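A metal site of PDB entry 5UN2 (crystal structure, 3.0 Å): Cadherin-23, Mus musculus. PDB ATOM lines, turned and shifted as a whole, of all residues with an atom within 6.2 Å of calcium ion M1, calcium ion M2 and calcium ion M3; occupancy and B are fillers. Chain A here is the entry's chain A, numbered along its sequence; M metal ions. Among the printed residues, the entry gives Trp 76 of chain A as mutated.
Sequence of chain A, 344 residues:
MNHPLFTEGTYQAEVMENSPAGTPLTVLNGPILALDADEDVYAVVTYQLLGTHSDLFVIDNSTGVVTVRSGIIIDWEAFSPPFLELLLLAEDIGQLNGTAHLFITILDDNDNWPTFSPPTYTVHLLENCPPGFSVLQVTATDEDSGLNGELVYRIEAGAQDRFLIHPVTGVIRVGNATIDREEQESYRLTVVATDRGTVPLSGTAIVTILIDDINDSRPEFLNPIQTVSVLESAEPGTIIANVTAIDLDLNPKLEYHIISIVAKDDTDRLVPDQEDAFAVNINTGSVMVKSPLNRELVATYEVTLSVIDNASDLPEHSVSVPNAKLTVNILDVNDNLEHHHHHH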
ATOM      1  N   GLU A  17     -18.598   8.149  20.254  1.00  0.00           N
ATOM      2  CA  GLU A  17     -19.824   8.202  21.054  1.00  0.00           C
ATOM      3  C   GLU A  17     -19.771   9.413  22.017  1.00  0.00           C
ATOM      4  O   GLU A  17     -18.672   9.843  22.386  1.00  0.00           O
ATOM      5  CB  GLU A  17     -20.064   6.868  21.814  1.00  0.00           C
ATOM      6  CG  GLU A  17     -19.034   6.517  22.911  1.00  0.00           C
ATOM      7  CD  GLU A  17     -19.509   5.457  23.921  1.00  0.00           C
ATOM      8  OE1 GLU A  17     -18.661   4.648  24.374  1.00  0.00           O
ATOM      9  OE2 GLU A  17     -20.716   5.432  24.285  1.00  0.00           O
ATOM     10  N   ASN A  18     -20.944   9.943  22.394  1.00  0.00           N
ATOM     11  CA  ASN A  18     -21.061  11.157  23.268  1.00  0.00           C
ATOM     12  C   ASN A  18     -20.517  12.482  22.665  1.00  0.00           C
ATOM     13  O   ASN A  18     -20.260  13.429  23.408  1.00  0.00           O
ATOM     14  CB  ASN A  18     -20.429  10.934  24.660  1.00  0.00           C
ATOM     15  CG  ASN A  18     -20.681   9.533  25.207  1.00  0.00           C
ATOM     16  OD1 ASN A  18     -21.815   9.045  25.202  1.00  0.00           O
ATOM     17  ND2 ASN A  18     -19.612   8.882  25.674  1.00  0.00           N
ATOM     18  N   ILE A  74     -25.236   9.649  21.013  1.00  0.00           N
ATOM     19  CA  ILE A  74     -24.602   8.480  20.373  1.00  0.00           C
ATOM     20  C   ILE A  74     -24.074   7.562  21.495  1.00  0.00           C
ATOM     21  O   ILE A  74     -23.191   7.969  22.258  1.00  0.00           O
ATOM     22  CB  ILE A  74     -23.389   8.882  19.479  1.00  0.00           C
ATOM     23  CG1 ILE A  74     -23.722   9.987  18.464  1.00  0.00           C
ATOM     24  CG2 ILE A  74     -22.815   7.673  18.770  1.00  0.00           C
ATOM     25  CD1 ILE A  74     -24.798   9.641  17.456  1.00  0.00           C
ATOM     26  N   ASP A  75     -24.606   6.338  21.596  1.00  0.00           N
ATOM     27  CA  ASP A  75     -24.241   5.368  22.653  1.00  0.00           C
ATOM     28  C   ASP A  75     -23.630   4.088  22.043  1.00  0.00           C
ATOM     29  O   ASP A  75     -24.349   3.280  21.445  1.00  0.00           O
ATOM     30  CB  ASP A  75     -25.507   5.043  23.465  1.00  0.00           C
ATOM     31  CG  ASP A  75     -25.210   4.351  24.780  1.00  0.00           C
ATOM     32  OD1 ASP A  75     -24.204   3.628  24.895  1.00  0.00           O
ATOM     33  OD2 ASP A  75     -26.009   4.531  25.706  1.00  0.00           O
ATOM     34  N   TRP A  76     -22.310   3.899  22.213  1.00  0.00           N
ATOM     35  CA  TRP A  76     -21.612   2.683  21.716  1.00  0.00           C
ATOM     36  C   TRP A  76     -22.215   1.413  22.288  1.00  0.00           C
ATOM     37  O   TRP A  76     -22.360   0.414  21.568  1.00  0.00           O
ATOM     38  CB  TRP A  76     -20.122   2.714  22.072  1.00  0.00           C
ATOM     39  CG  TRP A  76     -19.311   1.644  21.379  1.00  0.00           C
ATOM     40  CD1 TRP A  76     -18.649   1.772  20.222  1.00  0.00           C
ATOM     41  CD2 TRP A  76     -19.083   0.305  21.826  1.00  0.00           C
ATOM     42  NE1 TRP A  76     -18.011   0.607  19.900  1.00  0.00           N
ATOM     43  CE2 TRP A  76     -18.266  -0.321  20.868  1.00  0.00           C
ATOM     44  CE3 TRP A  76     -19.486  -0.441  22.941  1.00  0.00           C
ATOM     45  CZ2 TRP A  76     -17.852  -1.641  20.969  1.00  0.00           C
ATOM     46  CZ3 TRP A  76     -19.075  -1.757  23.052  1.00  0.00           C
ATOM     47  CH2 TRP A  76     -18.271  -2.344  22.062  1.00  0.00           C
ATOM     48  N   GLU A  77     -22.568   1.462  23.569  1.00  0.00           N
ATOM     49  CA  GLU A  77     -23.115   0.304  24.294  1.00  0.00           C
ATOM     50  C   GLU A  77     -24.537  -0.077  23.858  1.00  0.00           C
ATOM     51  O   GLU A  77     -24.994  -1.178  24.202  1.00  0.00           O
ATOM     52  CB  GLU A  77     -23.080   0.538  25.812  1.00  0.00           C
ATOM     53  CG  GLU A  77     -21.705   0.435  26.461  1.00  0.00           C
ATOM     54  CD  GLU A  77     -20.846   1.671  26.243  1.00  0.00           C
ATOM     55  OE1 GLU A  77     -21.317   2.808  26.506  1.00  0.00           O
ATOM     56  OE2 GLU A  77     -19.679   1.503  25.835  1.00  0.00           O
ATOM     57  N   ALA A  78     -25.225   0.809  23.118  1.00  0.00           N
ATOM     58  CA  ALA A  78     -26.583   0.572  22.619  1.00  0.00           C
ATOM     59  C   ALA A  78     -26.697  -0.032  21.187  1.00  0.00           C
ATOM     60  O   ALA A  78     -27.786  -0.417  20.768  1.00  0.00           O
ATOM     61  CB  ALA A  78     -27.389   1.863  22.711  1.00  0.00           C
ATOM     62  N   ASP A 108     -15.736   3.609  20.491  1.00  0.00           N
ATOM     63  CA  ASP A 108     -15.962   3.423  21.924  1.00  0.00           C
ATOM     64  C   ASP A 108     -15.195   4.473  22.718  1.00  0.00           C
ATOM     65  O   ASP A 108     -14.083   4.811  22.361  1.00  0.00           O
ATOM     66  CB  ASP A 108     -15.503   2.015  22.348  1.00  0.00           C
ATOM     67  CG  ASP A 108     -15.720   1.743  23.831  1.00  0.00           C
ATOM     68  OD1 ASP A 108     -16.714   2.239  24.393  1.00  0.00           O
ATOM     69  OD2 ASP A 108     -14.883   1.016  24.438  1.00  0.00           O
ATOM     70  N   ASP A 109     -15.821   4.995  23.780  1.00  0.00           N
ATOM     71  CA  ASP A 109     -15.122   5.855  24.757  1.00  0.00           C
ATOM     72  C   ASP A 109     -15.277   5.264  26.157  1.00  0.00           C
ATOM     73  O   ASP A 109     -16.302   4.648  26.467  1.00  0.00           O
ATOM     74  CB  ASP A 109     -15.665   7.294  24.734  1.00  0.00           C
ATOM     75  CG  ASP A 109     -14.853   8.241  25.630  1.00  0.00           C
ATOM     76  OD1 ASP A 109     -13.613   8.127  25.698  1.00  0.00           O
ATOM     77  OD2 ASP A 109     -15.470   9.106  26.280  1.00  0.00           O
ATOM     78  N   ASN A 110     -14.252   5.445  26.993  1.00  0.00           N
ATOM     79  CA  ASN A 110     -14.240   4.909  28.344  1.00  0.00           C
ATOM     80  C   ASN A 110     -15.246   5.680  29.192  1.00  0.00           C
ATOM     81  O   ASN A 110     -14.896   6.651  29.864  1.00  0.00           O
ATOM     82  CB  ASN A 110     -12.822   4.992  28.927  1.00  0.00           C
ATOM     83  CG  ASN A 110     -12.659   4.217  30.223  1.00  0.00           C
ATOM     84  OD1 ASN A 110     -13.461   3.342  30.554  1.00  0.00           O
ATOM     85  ND2 ASN A 110     -11.614   4.534  30.962  1.00  0.00           N
ATOM     86  N   ASP A 111     -16.509   5.260  29.128  1.00  0.00           N
ATOM     87  CA  ASP A 111     -17.607   5.967  29.793  1.00  0.00           C
ATOM     88  C   ASP A 111     -18.512   5.061  30.637  1.00  0.00           C
ATOM     89  O   ASP A 111     -19.681   5.393  30.873  1.00  0.00           O
ATOM     90  CB  ASP A 111     -18.437   6.752  28.757  1.00  0.00           C
ATOM     91  CG  ASP A 111     -19.197   5.846  27.769  1.00  0.00           C
ATOM     92  OD1 ASP A 111     -18.958   4.631  27.692  1.00  0.00           O
ATOM     93  OD2 ASP A 111     -20.048   6.384  27.046  1.00  0.00           O
ATOM     94  N   ASN A 112     -17.977   3.924  31.095  1.00  0.00           N
ATOM     95  CA  ASN A 112     -18.663   3.077  32.074  1.00  0.00           C
ATOM     96  C   ASN A 112     -17.706   2.771  33.219  1.00  0.00           C
ATOM     97  O   ASN A 112     -16.540   2.443  32.991  1.00  0.00           O
ATOM     98  CB  ASN A 112     -19.189   1.782  31.449  1.00  0.00           C
ATOM     99  CG  ASN A 112     -20.405   2.002  30.575  1.00  0.00           C
ATOM    100  OD1 ASN A 112     -21.512   1.591  30.941  1.00  0.00           O
ATOM    101  ND2 ASN A 112     -20.220   2.636  29.426  1.00  0.00           N
ATOM    102  N   TRP A 113     -18.226   2.879  34.434  1.00  0.00           N
ATOM    103  CA  TRP A 113     -17.442   2.750  35.652  1.00  0.00           C
ATOM    104  C   TRP A 113     -17.442   1.275  36.039  1.00  0.00           C
ATOM    105  O   TRP A 113     -18.508   0.653  36.011  1.00  0.00           O
ATOM    106  CB  TRP A 113     -18.053   3.602  36.773  1.00  0.00           C
ATOM    107  CG  TRP A 113     -18.020   5.078  36.475  1.00  0.00           C
ATOM    108  CD1 TRP A 113     -18.766   5.766  35.540  1.00  0.00           C
ATOM    109  CD2 TRP A 113     -17.193   6.063  37.112  1.00  0.00           C
ATOM    110  NE1 TRP A 113     -18.445   7.107  35.561  1.00  0.00           N
ATOM    111  CE2 TRP A 113     -17.482   7.313  36.514  1.00  0.00           C
ATOM    112  CE3 TRP A 113     -16.225   6.002  38.134  1.00  0.00           C
ATOM    113  CZ2 TRP A 113     -16.841   8.506  36.913  1.00  0.00           C
ATOM    114  CZ3 TRP A 113     -15.579   7.183  38.528  1.00  0.00           C
ATOM    115  CH2 TRP A 113     -15.897   8.426  37.924  1.00  0.00           C
ATOM    116  N   PRO A 114     -16.265   0.689  36.377  1.00  0.00           N
ATOM    117  CA  PRO A 114     -16.254  -0.698  36.855  1.00  0.00           C
ATOM    118  C   PRO A 114     -17.174  -0.869  38.039  1.00  0.00           C
ATOM    119  O   PRO A 114     -16.940  -0.269  39.069  1.00  0.00           O
ATOM    120  CB  PRO A 114     -14.784  -0.907  37.273  1.00  0.00           C
ATOM    121  CG  PRO A 114     -14.018   0.044  36.446  1.00  0.00           C
ATOM    122  CD  PRO A 114     -14.906   1.242  36.291  1.00  0.00           C
ATOM    123  N   ASP A 142     -18.023  -4.312  33.538  1.00  0.00           N
ATOM    124  CA  ASP A 142     -17.743  -3.097  32.773  1.00  0.00           C
ATOM    125  C   ASP A 142     -18.321  -3.251  31.343  1.00  0.00           C
ATOM    126  O   ASP A 142     -17.902  -4.151  30.579  1.00  0.00           O
ATOM    127  CB  ASP A 142     -16.234  -2.841  32.746  1.00  0.00           C
ATOM    128  CG  ASP A 142     -15.867  -1.413  32.416  1.00  0.00           C
ATOM    129  OD1 ASP A 142     -16.591  -0.746  31.645  1.00  0.00           O
ATOM    130  OD2 ASP A 142     -14.827  -0.940  32.918  1.00  0.00           O
ATOM    131  N   GLU A 143     -19.252  -2.367  31.002  1.00  0.00           N
ATOM    132  CA  GLU A 143     -19.913  -2.410  29.692  1.00  0.00           C
ATOM    133  C   GLU A 143     -19.105  -1.770  28.568  1.00  0.00           C
ATOM    134  O   GLU A 143     -19.548  -1.774  27.422  1.00  0.00           O
ATOM    135  CB  GLU A 143     -21.312  -1.781  29.751  1.00  0.00           C
ATOM    136  CG  GLU A 143     -22.215  -2.347  30.847  1.00  0.00           C
ATOM    137  CD  GLU A 143     -22.252  -3.864  30.867  1.00  0.00           C
ATOM    138  OE1 GLU A 143     -22.784  -4.477  29.918  1.00  0.00           O
ATOM    139  OE2 GLU A 143     -21.729  -4.450  31.846  1.00  0.00           O
ATOM    140  N   ASP A 144     -17.924  -1.232  28.883  1.00  0.00           N
ATOM    141  CA  ASP A 144     -16.993  -0.762  27.859  1.00  0.00           C
ATOM    142  C   ASP A 144     -16.319  -1.933  27.132  1.00  0.00           C
ATOM    143  O   ASP A 144     -16.490  -3.086  27.521  1.00  0.00           O
ATOM    144  CB  ASP A 144     -15.927   0.151  28.489  1.00  0.00           C
ATOM    145  CG  ASP A 144     -16.466   1.490  28.894  1.00  0.00           C
ATOM    146  OD1 ASP A 144     -17.241   2.075  28.107  1.00  0.00           O
ATOM    147  OD2 ASP A 144     -16.094   1.988  29.977  1.00  0.00           O
ATOM    148  N   SER A 145     -15.563  -1.588  26.082  1.00  0.00           N
ATOM    149  CA  SER A 145     -14.867  -2.557  25.232  1.00  0.00           C
ATOM    150  C   SER A 145     -13.357  -2.427  25.293  1.00  0.00           C
ATOM    151  O   SER A 145     -12.836  -1.343  25.587  1.00  0.00           O
ATOM    152  CB  SER A 145     -15.296  -2.381  23.777  1.00  0.00           C
ATOM    153  OG  SER A 145     -14.613  -1.285  23.167  1.00  0.00           O
ATOM    154  N   LEU A 147      -9.605  -2.340  26.194  1.00  0.00           N
ATOM    155  CA  LEU A 147      -8.922  -1.963  27.428  1.00  0.00           C
ATOM    156  C   LEU A 147      -9.815  -1.185  28.376  1.00  0.00           C
ATOM    157  O   LEU A 147      -9.595  -1.227  29.584  1.00  0.00           O
ATOM    158  CB  LEU A 147      -7.646  -1.183  27.139  1.00  0.00           C
ATOM    159  CG  LEU A 147      -6.472  -1.998  26.578  1.00  0.00           C
ATOM    160  CD1 LEU A 147      -5.317  -1.058  26.285  1.00  0.00           C
ATOM    161  CD2 LEU A 147      -6.047  -3.122  27.527  1.00  0.00           C
ATOM    162  N   ASN A 148     -10.825  -0.509  27.850  1.00  0.00           N
ATOM    163  CA  ASN A 148     -11.746   0.269  28.688  1.00  0.00           C
ATOM    164  C   ASN A 148     -12.674  -0.606  29.557  1.00  0.00           C
ATOM    165  O   ASN A 148     -13.310  -0.102  30.488  1.00  0.00           O
ATOM    166  CB  ASN A 148     -12.578   1.220  27.819  1.00  0.00           C
ATOM    167  CG  ASN A 148     -11.741   2.029  26.859  1.00  0.00           C
ATOM    168  OD1 ASN A 148     -10.622   2.479  27.170  1.00  0.00           O
ATOM    169  ND2 ASN A 148     -12.272   2.231  25.655  1.00  0.00           N
ATOM    170  N   GLY A 149     -12.782  -1.890  29.217  1.00  0.00           N
ATOM    171  CA  GLY A 149     -13.477  -2.896  30.023  1.00  0.00           C
ATOM    172  C   GLY A 149     -12.594  -3.825  30.831  1.00  0.00           C
ATOM    173  O   GLY A 149     -13.047  -4.387  31.830  1.00  0.00           O
ATOM    174  N   LEU A 151     -10.352  -5.010  33.536  1.00  0.00           N
ATOM    175  CA  LEU A 151     -10.291  -4.552  34.933  1.00  0.00           C
ATOM    176  C   LEU A 151      -9.098  -5.083  35.717  1.00  0.00           C
ATOM    177  O   LEU A 151      -8.664  -6.208  35.516  1.00  0.00           O
ATOM    178  CB  LEU A 151     -11.568  -4.951  35.682  1.00  0.00           C
ATOM    179  CG  LEU A 151     -12.925  -4.402  35.246  1.00  0.00           C
ATOM    180  CD1 LEU A 151     -13.980  -4.818  36.254  1.00  0.00           C
ATOM    181  CD2 LEU A 151     -12.904  -2.886  35.109  1.00  0.00           C
ATOM    182  N   ASP A 195     -10.357   0.318  35.532  1.00  0.00           N
ATOM    183  CA  ASP A 195     -10.208  -0.025  34.107  1.00  0.00           C
ATOM    184  C   ASP A 195      -8.862   0.483  33.548  1.00  0.00           C
ATOM    185  O   ASP A 195      -8.200   1.323  34.183  1.00  0.00           O
ATOM    186  CB  ASP A 195     -11.406   0.437  33.272  1.00  0.00           C
ATOM    187  CG  ASP A 195     -11.516   1.949  33.162  1.00  0.00           C
ATOM    188  OD1 ASP A 195     -10.635   2.591  32.570  1.00  0.00           O
ATOM    189  OD2 ASP A 195     -12.534   2.505  33.622  1.00  0.00           O
ATOM    190  N   LEU A 201     -11.284   4.914  34.786  1.00  0.00           N
ATOM    191  CA  LEU A 201     -12.267   4.973  35.863  1.00  0.00           C
ATOM    192  C   LEU A 201     -12.109   3.781  36.814  1.00  0.00           C
ATOM    193  O   LEU A 201     -11.501   2.766  36.463  1.00  0.00           O
ATOM    194  CB  LEU A 201     -13.690   5.045  35.281  1.00  0.00           C
ATOM    195  CG  LEU A 201     -13.911   6.128  34.209  1.00  0.00           C
ATOM    196  CD1 LEU A 201     -15.258   5.958  33.538  1.00  0.00           C
ATOM    197  CD2 LEU A 201     -13.770   7.525  34.805  1.00  0.00           C
HETATM  198 CA    CA M   1     -18.073   3.096  26.099  1.00  0.00          CA
HETATM  199 CA    CA M   2     -22.065   5.119  26.196  1.00  0.00          CA
HETATM  200 CA    CA M   3     -14.533   1.614  31.851  1.00  0.00          CA
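The nearest printed residue that does not touch calcium ion M2 is Asn 18 (4.1 Å).
ND2 of Asn 112 lies close to OE1 of Glu 77 (3.1 Å). The side-chain carboxylate (OD1) of Asp 75 is in hydrogen-bond range of the backbone NH (N) of Glu 77. OD2 of Asp 108 lies within hydrogen-bond range of ND2 of Asn 148 (3.1 Å). OD2 of Asp 108 is in hydrogen-bond range of OG of Ser 145 (2.6 Å). The side-chain carboxylate (OE2) of Glu 17 sits close to the backbone NH (N) of Trp 76, at 3.0 Å. OD1 of Asp 111 sits close to ND2 of Asn 112, 2.9 Å away. OD2 of Asp 111 sits close to ND2 of Asn 18 (2.9 Å). The backbone NH of Asp 195 is in hydrogen-bond range of the backbone carbonyl oxygen of Leu 201 (2.9 Å).
Six residues have an atom within 4 Å of calcium ion M3: Asn 110, Asn 112, Asp 142, Asp 144, Asn 148 and Asp 195. The nearest printed residue that does not touch calcium ion M3 is Pro 114 (4.5 Å).
Calcium ion M3 is bound by OD1 of Asn 110 (2.4 Å). Calcium ion M3 is bound by O of Asn 112 (2.5 Å). Calcium ion M3 is bound by OD2 of Asp 144, 2.5 Å away. Calcium ion M3 is bound by O of Asn 148 (2.5 Å). Calcium ion M3 is bound by OD2 of Asp 142, at 2.8 Å. Calcium ion M3 is bound by the side-chain carboxylate (OD2) of Asp 195. Slightly farther from calcium ion M3 lies the side-chain carboxylate (OD1) of Asp 142 (3.1 Å).
OE2 of Glu 77 is bound to calcium ion M1, at 2.3 Å. OD1 of Asp 108 binds calcium ion M1 (2.3 Å). OD1 of Asp 111 binds calcium ion M1. O of Asp 109 is bound to calcium ion M1, at 2.4 Å. OE1 of Glu 17 binds calcium ion M1 (2.4 Å). The side-chain carboxylate (OD1) of Asp 144 binds calcium ion M1.
Calcium ion M2 is bound by OE2 of Glu 17, 2.4 Å away. OE1 of Glu 77 is bound to calcium ion M2 (2.4 Å). The side-chain carboxylate (OD2) of Asp 111 is bound to calcium ion M2 (2.5 Å). Slightly farther from calcium ion M2 lies OD1 of Asp 75 (2.9 Å).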
